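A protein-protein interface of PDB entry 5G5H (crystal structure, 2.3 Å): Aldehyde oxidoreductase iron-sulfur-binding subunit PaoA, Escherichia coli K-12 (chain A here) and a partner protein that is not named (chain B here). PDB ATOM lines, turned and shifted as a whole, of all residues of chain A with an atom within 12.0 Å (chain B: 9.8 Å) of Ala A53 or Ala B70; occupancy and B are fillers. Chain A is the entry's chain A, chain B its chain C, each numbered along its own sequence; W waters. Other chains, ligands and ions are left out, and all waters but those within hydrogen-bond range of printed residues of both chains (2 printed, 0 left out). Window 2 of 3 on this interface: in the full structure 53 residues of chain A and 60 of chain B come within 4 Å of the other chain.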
ATOM      1  N   ALA A  53      -6.558   1.065  21.660  1.00  0.00           N
ATOM      2  CA  ALA A  53      -5.278   1.566  22.254  1.00  0.00           C
ATOM      3  C   ALA A  53      -5.234   3.092  22.443  1.00  0.00           C
ATOM      4  O   ALA A  53      -4.653   3.579  23.424  1.00  0.00           O
ATOM      5  CB  ALA A  53      -4.086   1.109  21.416  1.00  0.00           C
ATOM      6  N   ALA A  54      -5.817   3.835  21.498  1.00  0.00           N
ATOM      7  CA  ALA A  54      -5.775   5.309  21.495  1.00  0.00           C
ATOM      8  C   ALA A  54      -6.790   5.862  20.520  1.00  0.00           C
ATOM      9  O   ALA A  54      -7.298   5.129  19.681  1.00  0.00           O
ATOM     10  CB  ALA A  54      -4.379   5.815  21.117  1.00  0.00           C
ATOM     11  N   THR A  55      -7.082   7.152  20.647  1.00  0.00           N
ATOM     12  CA  THR A  55      -7.946   7.893  19.702  1.00  0.00           C
ATOM     13  C   THR A  55      -7.281   9.268  19.513  1.00  0.00           C
ATOM     14  O   THR A  55      -6.699   9.794  20.471  1.00  0.00           O
ATOM     15  CB  THR A  55      -9.423   8.020  20.204  1.00  0.00           C
ATOM     16  OG1 THR A  55     -10.283   8.554  19.174  1.00  0.00           O
ATOM     17  CG2 THR A  55      -9.512   8.909  21.451  1.00  0.00           C
ATOM     18  N   PRO A  56      -7.327   9.834  18.289  1.00  0.00           N
ATOM     19  CA  PRO A  56      -6.565  11.064  18.056  1.00  0.00           C
ATOM     20  C   PRO A  56      -7.163  12.321  18.701  1.00  0.00           C
ATOM     21  O   PRO A  56      -8.367  12.356  19.042  1.00  0.00           O
ATOM     22  CB  PRO A  56      -6.562  11.205  16.522  1.00  0.00           C
ATOM     23  CG  PRO A  56      -7.131   9.936  15.988  1.00  0.00           C
ATOM     24  CD  PRO A  56      -8.022   9.410  17.064  1.00  0.00           C
ATOM     25  N   ALA A  57      -6.300  13.332  18.855  1.00  0.00           N
ATOM     26  CA  ALA A  57      -6.681  14.627  19.431  1.00  0.00           C
ATOM     27  C   ALA A  57      -7.594  15.403  18.497  1.00  0.00           C
ATOM     28  O   ALA A  57      -7.519  15.244  17.286  1.00  0.00           O
ATOM     29  CB  ALA A  57      -5.451  15.463  19.764  1.00  0.00           C
ATOM     30  N   ARG A  79     -15.100  17.377  14.026  1.00  0.00           N
ATOM     31  CA  ARG A  79     -16.162  16.377  14.181  1.00  0.00           C
ATOM     32  C   ARG A  79     -17.521  16.967  14.510  1.00  0.00           C
ATOM     33  O   ARG A  79     -18.523  16.296  14.294  1.00  0.00           O
ATOM     34  CB  ARG A  79     -15.819  15.387  15.294  1.00  0.00           C
ATOM     35  CG  ARG A  79     -14.614  14.512  15.041  1.00  0.00           C
ATOM     36  CD  ARG A  79     -14.328  13.657  16.271  1.00  0.00           C
ATOM     37  NE  ARG A  79     -13.682  14.431  17.319  1.00  0.00           N
ATOM     38  CZ  ARG A  79     -13.064  13.925  18.384  1.00  0.00           C
ATOM     39  NH1 ARG A  79     -12.999  12.606  18.599  1.00  0.00           N
ATOM     40  NH2 ARG A  79     -12.500  14.763  19.254  1.00  0.00           N
ATOM     41  N   LEU B  66     -12.804  -4.501  33.691  1.00  0.00           N
ATOM     42  CA  LEU B  66     -13.192  -3.340  32.925  1.00  0.00           C
ATOM     43  C   LEU B  66     -11.996  -2.408  32.857  1.00  0.00           C
ATOM     44  O   LEU B  66     -11.603  -1.805  33.852  1.00  0.00           O
ATOM     45  CB  LEU B  66     -14.363  -2.645  33.588  1.00  0.00           C
ATOM     46  CG  LEU B  66     -14.969  -1.437  32.867  1.00  0.00           C
ATOM     47  CD1 LEU B  66     -15.135  -1.680  31.372  1.00  0.00           C
ATOM     48  CD2 LEU B  66     -16.328  -1.105  33.484  1.00  0.00           C
ATOM     49  N   ASP B  67     -11.413  -2.302  31.676  1.00  0.00           N
ATOM     50  CA  ASP B  67     -10.216  -1.516  31.491  1.00  0.00           C
ATOM     51  C   ASP B  67     -10.524  -0.102  31.029  1.00  0.00           C
ATOM     52  O   ASP B  67     -11.333   0.122  30.131  1.00  0.00           O
ATOM     53  CB  ASP B  67      -9.293  -2.231  30.536  1.00  0.00           C
ATOM     54  CG  ASP B  67      -8.671  -3.446  31.166  1.00  0.00           C
ATOM     55  OD1 ASP B  67      -7.895  -3.303  32.141  1.00  0.00           O
ATOM     56  OD2 ASP B  67      -8.976  -4.553  30.692  1.00  0.00           O
ATOM     57  N   THR B  68      -9.881   0.841  31.704  1.00  0.00           N
ATOM     58  CA  THR B  68     -10.135   2.252  31.546  1.00  0.00           C
ATOM     59  C   THR B  68      -8.878   3.094  31.290  1.00  0.00           C
ATOM     60  O   THR B  68      -9.015   4.292  31.100  1.00  0.00           O
ATOM     61  CB  THR B  68     -10.809   2.784  32.827  1.00  0.00           C
ATOM     62  OG1 THR B  68      -9.927   2.585  33.936  1.00  0.00           O
ATOM     63  CG2 THR B  68     -12.120   2.056  33.101  1.00  0.00           C
ATOM     64  N   ASP B  69      -7.676   2.496  31.284  1.00  0.00           N
ATOM     65  CA  ASP B  69      -6.430   3.253  31.092  1.00  0.00           C
ATOM     66  C   ASP B  69      -6.413   4.007  29.751  1.00  0.00           C
ATOM     67  O   ASP B  69      -6.093   5.203  29.707  1.00  0.00           O
ATOM     68  CB  ASP B  69      -5.174   2.356  31.165  1.00  0.00           C
ATOM     69  CG  ASP B  69      -4.633   2.140  32.595  1.00  0.00           C
ATOM     70  OD1 ASP B  69      -5.365   2.221  33.594  1.00  0.00           O
ATOM     71  OD2 ASP B  69      -3.419   1.846  32.706  1.00  0.00           O
ATOM     72  N   ALA B  70      -6.748   3.305  28.668  1.00  0.00           N
ATOM     73  CA  ALA B  70      -6.709   3.914  27.345  1.00  0.00           C
ATOM     74  C   ALA B  70      -7.674   5.090  27.254  1.00  0.00           C
ATOM     75  O   ALA B  70      -7.353   6.101  26.643  1.00  0.00           O
ATOM     76  CB  ALA B  70      -6.995   2.891  26.269  1.00  0.00           C
ATOM     77  N   ALA B  71      -8.838   4.959  27.885  1.00  0.00           N
ATOM     78  CA  ALA B  71      -9.839   6.021  27.917  1.00  0.00           C
ATOM     79  C   ALA B  71      -9.421   7.223  28.769  1.00  0.00           C
ATOM     80  O   ALA B  71      -9.615   8.363  28.378  1.00  0.00           O
ATOM     81  CB  ALA B  71     -11.158   5.459  28.422  1.00  0.00           C
ATOM     82  N   GLN B  72      -8.867   6.946  29.944  1.00  0.00           N
ATOM     83  CA  GLN B  72      -8.294   7.965  30.840  1.00  0.00           C
ATOM     84  C   GLN B  72      -7.235   8.823  30.141  1.00  0.00           C
ATOM     85  O   GLN B  72      -7.143  10.029  30.378  1.00  0.00           O
ATOM     86  CB  GLN B  72      -7.699   7.271  32.070  1.00  0.00           C
ATOM     87  CG  GLN B  72      -7.096   8.173  33.125  1.00  0.00           C
ATOM     88  CD  GLN B  72      -8.083   9.158  33.721  1.00  0.00           C
ATOM     89  OE1 GLN B  72      -9.230   8.818  34.006  1.00  0.00           O
ATOM     90  NE2 GLN B  72      -7.629  10.395  33.920  1.00  0.00           N
ATOM     91  N   LYS B  73      -6.456   8.198  29.271  1.00  0.00           N
ATOM     92  CA  LYS B  73      -5.353   8.863  28.568  1.00  0.00           C
ATOM     93  C   LYS B  73      -5.785   9.614  27.312  1.00  0.00           C
ATOM     94  O   LYS B  73      -5.017  10.415  26.775  1.00  0.00           O
ATOM     95  CB  LYS B  73      -4.280   7.844  28.191  1.00  0.00           C
ATOM     96  CG  LYS B  73      -3.523   7.315  29.387  1.00  0.00           C
ATOM     97  CD  LYS B  73      -2.284   6.528  28.986  1.00  0.00           C
ATOM     98  CE  LYS B  73      -2.653   5.278  28.212  1.00  0.00           C
ATOM     99  NZ  LYS B  73      -1.466   4.425  28.020  1.00  0.00           N
ATOM    100  N   ALA B  74      -7.011   9.367  26.868  1.00  0.00           N
ATOM    101  CA  ALA B  74      -7.547   9.984  25.670  1.00  0.00           C
ATOM    102  C   ALA B  74      -7.750  11.510  25.819  1.00  0.00           C
ATOM    103  O   ALA B  74      -7.856  12.021  26.933  1.00  0.00           O
ATOM    104  CB  ALA B  74      -8.850   9.290  25.286  1.00  0.00           C
ATOM    105  N   PRO B  75      -7.769  12.246  24.694  1.00  0.00           N
ATOM    106  CA  PRO B  75      -7.895  13.703  24.714  1.00  0.00           C
ATOM    107  C   PRO B  75      -9.112  14.270  25.462  1.00  0.00           C
ATOM    108  O   PRO B  75     -10.231  13.797  25.255  1.00  0.00           O
ATOM    109  CB  PRO B  75      -7.995  14.058  23.227  1.00  0.00           C
ATOM    110  CG  PRO B  75      -7.242  12.982  22.553  1.00  0.00           C
ATOM    111  CD  PRO B  75      -7.534  11.749  23.329  1.00  0.00           C
ATOM    112  N   GLY B  76      -8.865  15.284  26.301  1.00  0.00           N
ATOM    113  CA  GLY B  76      -9.880  15.979  27.110  1.00  0.00           C
ATOM    114  C   GLY B  76     -10.561  15.202  28.240  1.00  0.00           C
ATOM    115  O   GLY B  76     -11.570  15.682  28.799  1.00  0.00           O
ATOM    116  N   VAL B  77     -10.040  14.021  28.596  1.00  0.00           N
ATOM    117  CA  VAL B  77     -10.744  13.118  29.530  1.00  0.00           C
ATOM    118  C   VAL B  77     -10.392  13.433  30.987  1.00  0.00           C
ATOM    119  O   VAL B  77      -9.231  13.594  31.318  1.00  0.00           O
ATOM    120  CB  VAL B  77     -10.444  11.635  29.216  1.00  0.00           C
ATOM    121  CG1 VAL B  77     -10.898  10.717  30.340  1.00  0.00           C
ATOM    122  CG2 VAL B  77     -11.097  11.250  27.894  1.00  0.00           C
ATOM    123  N   ALA B  79     -12.232  11.658  33.867  1.00  0.00           N
ATOM    124  CA  ALA B  79     -12.399  10.452  34.682  1.00  0.00           C
ATOM    125  C   ALA B  79     -13.235   9.393  33.939  1.00  0.00           C
ATOM    126  O   ALA B  79     -13.902   9.702  32.958  1.00  0.00           O
ATOM    127  CB  ALA B  79     -13.068  10.806  36.003  1.00  0.00           C
ATOM    128  N   VAL B  80     -13.156   8.148  34.412  1.00  0.00           N
ATOM    129  CA  VAL B  80     -14.072   7.075  33.991  1.00  0.00           C
ATOM    130  C   VAL B  80     -14.726   6.523  35.235  1.00  0.00           C
ATOM    131  O   VAL B  80     -14.062   6.011  36.115  1.00  0.00           O
ATOM    132  CB  VAL B  80     -13.378   5.912  33.245  1.00  0.00           C
ATOM    133  CG1 VAL B  80     -14.415   5.072  32.506  1.00  0.00           C
ATOM    134  CG2 VAL B  80     -12.345   6.423  32.258  1.00  0.00           C
ATOM    135  N   VAL B 115     -17.463   7.800  30.660  1.00  0.00           N
ATOM    136  CA  VAL B 115     -16.266   8.598  30.435  1.00  0.00           C
ATOM    137  C   VAL B 115     -16.662  10.058  30.513  1.00  0.00           C
ATOM    138  O   VAL B 115     -17.523  10.492  29.771  1.00  0.00           O
ATOM    139  CB  VAL B 115     -15.625   8.295  29.072  1.00  0.00           C
ATOM    140  CG1 VAL B 115     -14.277   9.004  28.950  1.00  0.00           C
ATOM    141  CG2 VAL B 115     -15.439   6.787  28.906  1.00  0.00           C
ATOM    142  N   GLN B 122     -15.041  14.413  22.500  1.00  0.00           N
ATOM    143  CA  GLN B 122     -13.959  13.742  23.217  1.00  0.00           C
ATOM    144  C   GLN B 122     -14.438  12.598  24.125  1.00  0.00           C
ATOM    145  O   GLN B 122     -13.754  11.579  24.248  1.00  0.00           O
ATOM    146  CB  GLN B 122     -13.123  14.759  24.006  1.00  0.00           C
ATOM    147  CG  GLN B 122     -12.189  15.540  23.100  1.00  0.00           C
ATOM    148  CD  GLN B 122     -11.341  16.597  23.806  1.00  0.00           C
ATOM    149  OE1 GLN B 122     -10.098  16.600  23.693  1.00  0.00           O
ATOM    150  NE2 GLN B 122     -12.000  17.507  24.521  1.00  0.00           N
ATOM    151  N   ALA B 123     -15.598  12.767  24.757  1.00  0.00           N
ATOM    152  CA  ALA B 123     -16.140  11.751  25.642  1.00  0.00           C
ATOM    153  C   ALA B 123     -16.605  10.501  24.880  1.00  0.00           C
ATOM    154  O   ALA B 123     -16.398   9.375  25.329  1.00  0.00           O
ATOM    155  CB  ALA B 123     -17.286  12.320  26.458  1.00  0.00           C
ATOM    156  N   ALA B 125     -15.537   9.531  21.798  1.00  0.00           N
ATOM    157  CA  ALA B 125     -14.377   8.879  21.222  1.00  0.00           C
ATOM    158  C   ALA B 125     -13.636   8.100  22.297  1.00  0.00           C
ATOM    159  O   ALA B 125     -13.170   6.976  22.057  1.00  0.00           O
ATOM    160  CB  ALA B 125     -13.456   9.902  20.579  1.00  0.00           C
ATOM    161  N   ALA B 126     -13.538   8.704  23.479  1.00  0.00           N
ATOM    162  CA  ALA B 126     -12.895   8.066  24.617  1.00  0.00           C
ATOM    163  C   ALA B 126     -13.661   6.840  25.126  1.00  0.00           C
ATOM    164  O   ALA B 126     -13.051   5.835  25.494  1.00  0.00           O
ATOM    165  CB  ALA B 126     -12.678   9.074  25.738  1.00  0.00           C
ATOM    166  N   ALA B 127     -14.990   6.913  25.124  1.00  0.00           N
ATOM    167  CA  ALA B 127     -15.828   5.764  25.505  1.00  0.00           C
ATOM    168  C   ALA B 127     -15.562   4.518  24.669  1.00  0.00           C
ATOM    169  O   ALA B 127     -15.636   3.428  25.200  1.00  0.00           O
ATOM    170  CB  ALA B 127     -17.304   6.118  25.462  1.00  0.00           C
ATOM    171  N   SER B 128     -15.229   4.678  23.387  1.00  0.00           N
ATOM    172  CA  SER B 128     -14.873   3.546  22.515  1.00  0.00           C
ATOM    173  C   SER B 128     -13.612   2.791  22.943  1.00  0.00           C
ATOM    174  O   SER B 128     -13.387   1.686  22.485  1.00  0.00           O
ATOM    175  CB  SER B 128     -14.661   4.010  21.067  1.00  0.00           C
ATOM    176  OG  SER B 128     -15.592   5.014  20.700  1.00  0.00           O
ATOM    177  N   LEU B 129     -12.769   3.406  23.769  1.00  0.00           N
ATOM    178  CA  LEU B 129     -11.529   2.785  24.248  1.00  0.00           C
ATOM    179  C   LEU B 129     -11.730   1.976  25.541  1.00  0.00           C
ATOM    180  O   LEU B 129     -10.839   1.218  25.941  1.00  0.00           O
ATOM    181  CB  LEU B 129     -10.486   3.863  24.500  1.00  0.00           C
ATOM    182  CG  LEU B 129     -10.231   4.855  23.366  1.00  0.00           C
ATOM    183  CD1 LEU B 129      -9.115   5.803  23.761  1.00  0.00           C
ATOM    184  CD2 LEU B 129      -9.876   4.140  22.073  1.00  0.00           C
ATOM    185  N   VAL B 130     -12.882   2.135  26.200  1.00  0.00           N
ATOM    186  CA  VAL B 130     -13.168   1.352  27.400  1.00  0.00           C
ATOM    187  C   VAL B 130     -13.308  -0.129  26.980  1.00  0.00           C
ATOM    188  O   VAL B 130     -14.132  -0.452  26.143  1.00  0.00           O
ATOM    189  CB  VAL B 130     -14.416   1.879  28.141  1.00  0.00           C
ATOM    190  CG1 VAL B 130     -14.782   0.986  29.325  1.00  0.00           C
ATOM    191  CG2 VAL B 130     -14.182   3.314  28.621  1.00  0.00           C
ATOM    192  N   GLN B 131     -12.466  -0.996  27.539  1.00  0.00           N
ATOM    193  CA  GLN B 131     -12.389  -2.413  27.154  1.00  0.00           C
ATOM    194  C   GLN B 131     -12.958  -3.286  28.273  1.00  0.00           C
ATOM    195  O   GLN B 131     -12.298  -3.488  29.287  1.00  0.00           O
ATOM    196  CB  GLN B 131     -10.924  -2.809  26.912  1.00  0.00           C
ATOM    197  CG  GLN B 131     -10.217  -2.137  25.742  1.00  0.00           C
ATOM    198  CD  GLN B 131      -8.675  -2.125  25.884  1.00  0.00           C
ATOM    199  OE1 GLN B 131      -8.003  -3.176  25.835  1.00  0.00           O
ATOM    200  NE2 GLN B 131      -8.111  -0.925  26.035  1.00  0.00           N
HETATM  201  O   HOH W   1     -12.263   6.643  19.361  1.00  0.00           O
HETATM  202  O   HOH W   2      -5.018   6.287  25.033  1.00  0.00           O
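Of chain B, only Ala B70 comes within 4 Å of Ala A53.
Of chain A, only Ala A53 comes within 4 Å of Ala B70.
Ala A54 touches just one residue of chain B: Leu B129 (3.7 Å).
No residue of chain A comes within 4 Å of Asp B69.
No residue of chain A comes within 4 Å of Ala B126.
Printed residues of chain A within 4 Å of Leu B129: Ala A54 and Thr A55.
Of the printed residues of chain B, Thr A55 touches Ala B74 (3.9 Å), Pro B75 (3.6 Å), Ala B125 (3.7 Å) and Leu B129 (3.9 Å).
Printed residues of chain B within 4 Å of Ala A57: Pro B75 (3.6 Å).
Of the printed residues of chain A, Gln B122 touches Arg A79.
Printed residues of chain A within 4 Å of Pro B75: Thr A55 (3.6 Å), Pro A56 (3.7 Å) and Ala A57 (3.6 Å).
Of the printed residues of chain B, Pro A56 touches Pro B75 (3.7 Å).
Ala B79 touches none of the printed residues of chain A.
Val B130 touches none of the printed residues of chain A.
The nearest residue of chain B that does not touch Ala A53 is Leu B129 (4.5 Å).
The nearest residue of chain A that does not touch Ala B70 is Ala A54 (5.0 Å).
CB of Ala B70 touches O of Ala A53 (3.7 Å).
O of Ala A54 touches CD2 of Leu B129 (3.7 Å).
CB of Ala B74 touches CG2 of Thr A55, 3.9 Å away.
CD of Pro B75 touches O of Thr A55, at 3.6 Å.
OG1 of Thr A55 touches CB of Ala B125, at 3.7 Å.
Leu B129 touches Thr A55.
CG of Pro B75 touches O of Pro A56, 3.7 Å away.
CA of Ala A57 touches CG of Pro B75 (3.6 Å).
Gln B122 touches Arg A79.
Ala B125 touches Arg A79 (CB to NH1, 3.4 Å).
Water W1 bridges the side-chain hydroxyl of Thr A55 and the backbone carbonyl oxygen of Ala B125.
Water W2 bridges the backbone carbonyl oxygen of Ala B70 (2.8 Å) and the backbone carbonyl oxygen of Ala A53 (3.2 Å).
Printed residues of chain B that touch a printed residue of chain A: Ala B70, Ala B74, Pro B75, Gln B122, Ala B125 and Leu B129.
Along chain B the printed residues that touch a printed residue of chain A span positions 70 to 129.
Among the printed residues, no Asp or Glu carboxylate lies within 4 Å of a Lys or Arg side-chain nitrogen of the other chain.
OE1 of Gln B122 lies close to O of Pro B75 (3.2 Å).
The side-chain amide oxygen of Gln B122 is in hydrogen-bond range of the backbone NH of Gly B76.
The backbone carbonyl oxygen (O) of Leu B129 lies close to the side-chain amide nitrogen (NE2) of Gln B131 (3.5 Å).
The side-chain hydroxyl of Ser B128 sits at hydrogen-bond distance from the backbone carbonyl oxygen of Ala B125, 3.4 Å away.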
